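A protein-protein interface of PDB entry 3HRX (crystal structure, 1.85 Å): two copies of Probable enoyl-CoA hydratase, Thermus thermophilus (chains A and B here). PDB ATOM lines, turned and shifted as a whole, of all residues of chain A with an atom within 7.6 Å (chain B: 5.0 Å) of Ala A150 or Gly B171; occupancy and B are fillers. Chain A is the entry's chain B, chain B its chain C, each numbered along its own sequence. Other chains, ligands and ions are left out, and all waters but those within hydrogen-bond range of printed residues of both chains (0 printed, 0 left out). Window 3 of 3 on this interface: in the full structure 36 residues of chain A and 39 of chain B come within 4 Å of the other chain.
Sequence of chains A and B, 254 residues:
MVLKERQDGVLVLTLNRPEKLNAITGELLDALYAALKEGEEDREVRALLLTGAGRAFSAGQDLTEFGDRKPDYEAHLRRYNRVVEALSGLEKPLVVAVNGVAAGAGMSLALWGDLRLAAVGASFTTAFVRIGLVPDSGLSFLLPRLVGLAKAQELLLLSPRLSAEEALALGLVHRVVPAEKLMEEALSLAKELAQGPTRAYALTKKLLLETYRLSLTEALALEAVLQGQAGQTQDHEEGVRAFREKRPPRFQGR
The backbone carbonyl oxygen of Arg B145 lies within hydrogen-bond range of the backbone NH of Leu A149, 3.0 Å away.
A ring nitrogen (NE2) of His B174 lies within hydrogen-bond range of the backbone carbonyl oxygen (O) of Ala A150 (3.0 Å).
The side-chain amide oxygen of Gln A153 is in hydrogen-bond range of the guanidinium group of Arg B116, 2.9 Å away.
Hydrophobic or aromatic side chains of chain B within 4 Å of the printed part of chain A: Leu B146 and His B174.
Hydrophobic or aromatic side chains of chain A within 4 Å of the printed part of chain B: Leu A149 and Ala A150.
Along chain A the printed residues that touch a printed residue of chain B span positions 149 to 154.
Among the printed residues, 10 pairs touch across the chains.
The side-chain carboxylate (OE1) of Glu A154 lies within salt-bridge range of the side-chain amino group (NZ) of Lys A151, 2.8 Å away.
The guanidinium group (NH2) of Arg B116 is in hydrogen-bond range of the backbone carbonyl oxygen (O) of Gly B171.
O of Leu B172 sits at hydrogen-bond distance from NE of Arg B116 (2.6 Å).
O of Arg B116 sits at hydrogen-bond distance from N of His B174 (2.6 Å).
Of chain B, only Arg B116 (3.6 Å), Leu B146 (3.6 Å), Gly B171 (3.2 Å) and His B174 (3.0 Å) come within 4 Å of Ala A150.
Of the printed residues of chain B, Glu A154 touches His B174 (3.7 Å).
Of the printed residues of chain A, Leu B146 touches Leu A149, Ala A150 and Gln A153.
Gly B171 touches just one residue of chain A: Ala A150.
Position printed for both chains: 147.
Of the 10 pairs that touch across the chains among the printed residues, none has its exchanged pair printed and touching as well.
Leu A149 touches Leu B146.
Ala A150 touches Arg B116 (CB to NH2, 3.6 Å).
Leu B146 touches Ala A150.
Ala A150 touches Gly B171.
CD2 of Leu B146 touches OE1 of Gln A153, at 3.8 Å.
Gln A153 touches His B174 (OE1 to CE1, 3.9 Å).
His B174 touches Glu A154.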
ATOM      1  N   PRO A 144     -16.230 -18.167   8.301  1.00  0.00           N
ATOM      2  CA  PRO A 144     -16.516 -19.572   7.989  1.00  0.00           C
ATOM      3  C   PRO A 144     -17.852 -20.028   8.579  1.00  0.00           C
ATOM      4  O   PRO A 144     -18.607 -20.755   7.942  1.00  0.00           O
ATOM      5  CB  PRO A 144     -15.338 -20.323   8.620  1.00  0.00           C
ATOM      6  CG  PRO A 144     -14.250 -19.300   8.675  1.00  0.00           C
ATOM      7  CD  PRO A 144     -14.976 -18.047   9.066  1.00  0.00           C
ATOM      8  N   VAL A 147     -20.804 -18.094   6.419  1.00  0.00           N
ATOM      9  CA  VAL A 147     -20.989 -18.438   5.009  1.00  0.00           C
ATOM     10  C   VAL A 147     -20.470 -19.805   4.580  1.00  0.00           C
ATOM     11  O   VAL A 147     -20.650 -20.205   3.430  1.00  0.00           O
ATOM     12  CB  VAL A 147     -20.322 -17.383   4.095  1.00  0.00           C
ATOM     13  CG1 VAL A 147     -20.892 -16.008   4.381  1.00  0.00           C
ATOM     14  CG2 VAL A 147     -18.810 -17.390   4.304  1.00  0.00           C
ATOM     15  N   GLY A 148     -19.825 -20.519   5.492  1.00  0.00           N
ATOM     16  CA  GLY A 148     -19.287 -21.821   5.140  1.00  0.00           C
ATOM     17  C   GLY A 148     -17.825 -21.685   4.759  1.00  0.00           C
ATOM     18  O   GLY A 148     -17.393 -20.628   4.296  1.00  0.00           O
ATOM     19  N   LEU A 149     -17.058 -22.755   4.940  1.00  0.00           N
ATOM     20  CA  LEU A 149     -15.632 -22.723   4.634  1.00  0.00           C
ATOM     21  C   LEU A 149     -15.316 -22.452   3.169  1.00  0.00           C
ATOM     22  O   LEU A 149     -14.397 -21.692   2.859  1.00  0.00           O
ATOM     23  CB  LEU A 149     -14.971 -24.041   5.054  1.00  0.00           C
ATOM     24  CG  LEU A 149     -13.461 -24.122   4.803  1.00  0.00           C
ATOM     25  CD1 LEU A 149     -12.758 -22.986   5.545  1.00  0.00           C
ATOM     26  CD2 LEU A 149     -12.929 -25.475   5.267  1.00  0.00           C
ATOM     27  N   ALA A 150     -16.063 -23.077   2.266  1.00  0.00           N
ATOM     28  CA  ALA A 150     -15.811 -22.894   0.840  1.00  0.00           C
ATOM     29  C   ALA A 150     -15.823 -21.416   0.456  1.00  0.00           C
ATOM     30  O   ALA A 150     -14.874 -20.922  -0.154  1.00  0.00           O
ATOM     31  CB  ALA A 150     -16.842 -23.670   0.014  1.00  0.00           C
ATOM     32  N   LYS A 151     -16.890 -20.709   0.816  1.00  0.00           N
ATOM     33  CA  LYS A 151     -16.992 -19.289   0.499  1.00  0.00           C
ATOM     34  C   LYS A 151     -15.999 -18.454   1.304  1.00  0.00           C
ATOM     35  O   LYS A 151     -15.450 -17.478   0.796  1.00  0.00           O
ATOM     36  CB  LYS A 151     -18.417 -18.780   0.747  1.00  0.00           C
ATOM     37  CG  LYS A 151     -19.471 -19.438  -0.131  1.00  0.00           C
ATOM     38  CD  LYS A 151     -19.149 -19.309  -1.614  1.00  0.00           C
ATOM     39  CE  LYS A 151     -19.108 -17.862  -2.068  1.00  0.00           C
ATOM     40  NZ  LYS A 151     -18.863 -17.764  -3.537  1.00  0.00           N
ATOM     41  N   ALA A 152     -15.765 -18.825   2.558  1.00  0.00           N
ATOM     42  CA  ALA A 152     -14.812 -18.075   3.373  1.00  0.00           C
ATOM     43  C   ALA A 152     -13.432 -18.090   2.703  1.00  0.00           C
ATOM     44  O   ALA A 152     -12.754 -17.062   2.631  1.00  0.00           O
ATOM     45  CB  ALA A 152     -14.725 -18.674   4.777  1.00  0.00           C
ATOM     46  N   GLN A 153     -13.024 -19.257   2.208  1.00  0.00           N
ATOM     47  CA  GLN A 153     -11.731 -19.394   1.536  1.00  0.00           C
ATOM     48  C   GLN A 153     -11.623 -18.424   0.375  1.00  0.00           C
ATOM     49  O   GLN A 153     -10.638 -17.697   0.236  1.00  0.00           O
ATOM     50  CB  GLN A 153     -11.556 -20.806   0.978  1.00  0.00           C
ATOM     51  CG  GLN A 153     -11.498 -21.897   2.004  1.00  0.00           C
ATOM     52  CD  GLN A 153     -11.446 -23.267   1.360  1.00  0.00           C
ATOM     53  OE1 GLN A 153     -12.277 -23.599   0.511  1.00  0.00           O
ATOM     54  NE2 GLN A 153     -10.474 -24.072   1.762  1.00  0.00           N
ATOM     55  N   GLU A 154     -12.646 -18.435  -0.468  1.00  0.00           N
ATOM     56  CA  GLU A 154     -12.676 -17.577  -1.638  1.00  0.00           C
ATOM     57  C   GLU A 154     -12.701 -16.093  -1.283  1.00  0.00           C
ATOM     58  O   GLU A 154     -11.911 -15.315  -1.820  1.00  0.00           O
ATOM     59  CB  GLU A 154     -13.881 -17.944  -2.507  1.00  0.00           C
ATOM     60  CG  GLU A 154     -14.096 -17.034  -3.699  1.00  0.00           C
ATOM     61  CD  GLU A 154     -15.191 -17.541  -4.617  1.00  0.00           C
ATOM     62  OE1 GLU A 154     -16.186 -18.100  -4.105  1.00  0.00           O
ATOM     63  OE2 GLU A 154     -15.065 -17.371  -5.847  1.00  0.00           O
ATOM     64  N   LEU A 155     -13.598 -15.702  -0.379  1.00  0.00           N
ATOM     65  CA  LEU A 155     -13.709 -14.300   0.027  1.00  0.00           C
ATOM     66  C   LEU A 155     -12.442 -13.753   0.673  1.00  0.00           C
ATOM     67  O   LEU A 155     -12.071 -12.601   0.448  1.00  0.00           O
ATOM     68  CB  LEU A 155     -14.886 -14.109   0.995  1.00  0.00           C
ATOM     69  CG  LEU A 155     -16.278 -13.860   0.406  1.00  0.00           C
ATOM     70  CD1 LEU A 155     -16.560 -14.846  -0.704  1.00  0.00           C
ATOM     71  CD2 LEU A 155     -17.325 -13.963   1.511  1.00  0.00           C
ATOM     72  N   LEU A 156     -11.778 -14.575   1.478  1.00  0.00           N
ATOM     73  CA  LEU A 156     -10.566 -14.145   2.164  1.00  0.00           C
ATOM     74  C   LEU A 156      -9.315 -14.141   1.289  1.00  0.00           C
ATOM     75  O   LEU A 156      -8.519 -13.204   1.340  1.00  0.00           O
ATOM     76  CB  LEU A 156     -10.320 -15.030   3.388  1.00  0.00           C
ATOM     77  CG  LEU A 156     -11.307 -14.870   4.546  1.00  0.00           C
ATOM     78  CD1 LEU A 156     -11.066 -15.954   5.587  1.00  0.00           C
ATOM     79  CD2 LEU A 156     -11.142 -13.487   5.166  1.00  0.00           C
ATOM     80  N   ARG B 116     -10.824 -24.210  -5.890  1.00  0.00           N
ATOM     81  CA  ARG B 116     -11.090 -25.394  -6.678  1.00  0.00           C
ATOM     82  C   ARG B 116     -11.914 -25.114  -7.926  1.00  0.00           C
ATOM     83  O   ARG B 116     -12.943 -24.438  -7.871  1.00  0.00           O
ATOM     84  CB  ARG B 116     -11.801 -26.421  -5.789  1.00  0.00           C
ATOM     85  CG  ARG B 116     -11.043 -26.726  -4.492  1.00  0.00           C
ATOM     86  CD  ARG B 116     -11.859 -27.612  -3.552  1.00  0.00           C
ATOM     87  NE  ARG B 116     -13.055 -26.932  -3.060  1.00  0.00           N
ATOM     88  CZ  ARG B 116     -13.061 -26.010  -2.104  1.00  0.00           C
ATOM     89  NH1 ARG B 116     -11.930 -25.644  -1.513  1.00  0.00           N
ATOM     90  NH2 ARG B 116     -14.206 -25.447  -1.738  1.00  0.00           N
ATOM     91  N   ARG B 145     -17.558 -28.862   6.901  1.00  0.00           N
ATOM     92  CA  ARG B 145     -17.124 -27.477   6.983  1.00  0.00           C
ATOM     93  C   ARG B 145     -17.388 -26.757   5.657  1.00  0.00           C
ATOM     94  O   ARG B 145     -17.848 -25.615   5.639  1.00  0.00           O
ATOM     95  CB  ARG B 145     -15.630 -27.415   7.330  1.00  0.00           C
ATOM     96  CG  ARG B 145     -15.308 -27.929   8.734  1.00  0.00           C
ATOM     97  CD  ARG B 145     -13.807 -27.959   8.991  1.00  0.00           C
ATOM     98  NE  ARG B 145     -13.479 -28.165  10.405  1.00  0.00           N
ATOM     99  CZ  ARG B 145     -13.764 -29.262  11.101  1.00  0.00           C
ATOM    100  NH1 ARG B 145     -14.391 -30.282  10.527  1.00  0.00           N
ATOM    101  NH2 ARG B 145     -13.412 -29.343  12.380  1.00  0.00           N
ATOM    102  N   LEU B 146     -17.117 -27.441   4.550  1.00  0.00           N
ATOM    103  CA  LEU B 146     -17.301 -26.856   3.225  1.00  0.00           C
ATOM    104  C   LEU B 146     -18.745 -26.640   2.785  1.00  0.00           C
ATOM    105  O   LEU B 146     -19.086 -25.565   2.289  1.00  0.00           O
ATOM    106  CB  LEU B 146     -16.592 -27.712   2.168  1.00  0.00           C
ATOM    107  CG  LEU B 146     -15.062 -27.713   2.196  1.00  0.00           C
ATOM    108  CD1 LEU B 146     -14.534 -28.776   1.243  1.00  0.00           C
ATOM    109  CD2 LEU B 146     -14.537 -26.336   1.818  1.00  0.00           C
ATOM    110  N   VAL B 147     -19.590 -27.653   2.967  1.00  0.00           N
ATOM    111  CA  VAL B 147     -20.982 -27.565   2.529  1.00  0.00           C
ATOM    112  C   VAL B 147     -22.045 -27.610   3.625  1.00  0.00           C
ATOM    113  O   VAL B 147     -23.245 -27.586   3.329  1.00  0.00           O
ATOM    114  CB  VAL B 147     -21.297 -28.689   1.525  1.00  0.00           C
ATOM    115  CG1 VAL B 147     -20.314 -28.633   0.363  1.00  0.00           C
ATOM    116  CG2 VAL B 147     -21.221 -30.050   2.218  1.00  0.00           C
ATOM    117  N   ALA B 167     -21.847 -29.292  -7.839  1.00  0.00           N
ATOM    118  CA  ALA B 167     -20.713 -29.109  -6.938  1.00  0.00           C
ATOM    119  C   ALA B 167     -20.470 -27.610  -6.768  1.00  0.00           C
ATOM    120  O   ALA B 167     -20.116 -27.142  -5.683  1.00  0.00           O
ATOM    121  CB  ALA B 167     -19.463 -29.786  -7.515  1.00  0.00           C
ATOM    122  N   LEU B 168     -20.669 -26.857  -7.846  1.00  0.00           N
ATOM    123  CA  LEU B 168     -20.474 -25.409  -7.819  1.00  0.00           C
ATOM    124  C   LEU B 168     -21.498 -24.722  -6.919  1.00  0.00           C
ATOM    125  O   LEU B 168     -21.162 -23.814  -6.156  1.00  0.00           O
ATOM    126  CB  LEU B 168     -20.576 -24.839  -9.233  1.00  0.00           C
ATOM    127  CG  LEU B 168     -20.464 -23.320  -9.368  1.00  0.00           C
ATOM    128  CD1 LEU B 168     -19.118 -22.841  -8.839  1.00  0.00           C
ATOM    129  CD2 LEU B 168     -20.630 -22.939 -10.829  1.00  0.00           C
ATOM    130  N   ALA B 169     -22.749 -25.155  -7.016  1.00  0.00           N
ATOM    131  CA  ALA B 169     -23.814 -24.585  -6.202  1.00  0.00           C
ATOM    132  C   ALA B 169     -23.564 -24.823  -4.714  1.00  0.00           C
ATOM    133  O   ALA B 169     -23.848 -23.964  -3.883  1.00  0.00           O
ATOM    134  CB  ALA B 169     -25.158 -25.194  -6.605  1.00  0.00           C
ATOM    135  N   LEU B 170     -23.033 -25.996  -4.383  1.00  0.00           N
ATOM    136  CA  LEU B 170     -22.775 -26.355  -2.993  1.00  0.00           C
ATOM    137  C   LEU B 170     -21.479 -25.781  -2.432  1.00  0.00           C
ATOM    138  O   LEU B 170     -21.338 -25.627  -1.220  1.00  0.00           O
ATOM    139  CB  LEU B 170     -22.759 -27.880  -2.840  1.00  0.00           C
ATOM    140  CG  LEU B 170     -24.029 -28.618  -3.281  1.00  0.00           C
ATOM    141  CD1 LEU B 170     -23.843 -30.109  -3.077  1.00  0.00           C
ATOM    142  CD2 LEU B 170     -25.230 -28.112  -2.492  1.00  0.00           C
ATOM    143  N   GLY B 171     -20.530 -25.474  -3.308  1.00  0.00           N
ATOM    144  CA  GLY B 171     -19.265 -24.933  -2.847  1.00  0.00           C
ATOM    145  C   GLY B 171     -18.124 -25.930  -2.934  1.00  0.00           C
ATOM    146  O   GLY B 171     -16.994 -25.619  -2.554  1.00  0.00           O
ATOM    147  N   LEU B 172     -18.403 -27.138  -3.418  1.00  0.00           N
ATOM    148  CA  LEU B 172     -17.345 -28.132  -3.547  1.00  0.00           C
ATOM    149  C   LEU B 172     -16.272 -27.568  -4.478  1.00  0.00           C
ATOM    150  O   LEU B 172     -15.097 -27.912  -4.362  1.00  0.00           O
ATOM    151  CB  LEU B 172     -17.902 -29.451  -4.087  1.00  0.00           C
ATOM    152  CG  LEU B 172     -18.827 -30.193  -3.117  1.00  0.00           C
ATOM    153  CD1 LEU B 172     -19.370 -31.445  -3.788  1.00  0.00           C
ATOM    154  CD2 LEU B 172     -18.064 -30.550  -1.842  1.00  0.00           C
ATOM    155  N   VAL B 173     -16.684 -26.713  -5.412  1.00  0.00           N
ATOM    156  CA  VAL B 173     -15.741 -26.051  -6.311  1.00  0.00           C
ATOM    157  C   VAL B 173     -16.160 -24.595  -6.389  1.00  0.00           C
ATOM    158  O   VAL B 173     -17.308 -24.260  -6.093  1.00  0.00           O
ATOM    159  CB  VAL B 173     -15.709 -26.674  -7.734  1.00  0.00           C
ATOM    160  CG1 VAL B 173     -15.283 -28.127  -7.642  1.00  0.00           C
ATOM    161  CG2 VAL B 173     -17.065 -26.536  -8.421  1.00  0.00           C
ATOM    162  N   HIS B 174     -15.229 -23.729  -6.767  1.00  0.00           N
ATOM    163  CA  HIS B 174     -15.504 -22.303  -6.845  1.00  0.00           C
ATOM    164  C   HIS B 174     -15.836 -21.839  -8.255  1.00  0.00           C
ATOM    165  O   HIS B 174     -16.417 -20.772  -8.443  1.00  0.00           O
ATOM    166  CB  HIS B 174     -14.307 -21.508  -6.314  1.00  0.00           C
ATOM    167  CG  HIS B 174     -13.954 -21.822  -4.892  1.00  0.00           C
ATOM    168  ND1 HIS B 174     -12.983 -22.737  -4.548  1.00  0.00           N
ATOM    169  CD2 HIS B 174     -14.451 -21.344  -3.726  1.00  0.00           C
ATOM    170  CE1 HIS B 174     -12.894 -22.808  -3.231  1.00  0.00           C
ATOM    171  NE2 HIS B 174     -13.775 -21.973  -2.709  1.00  0.00           N
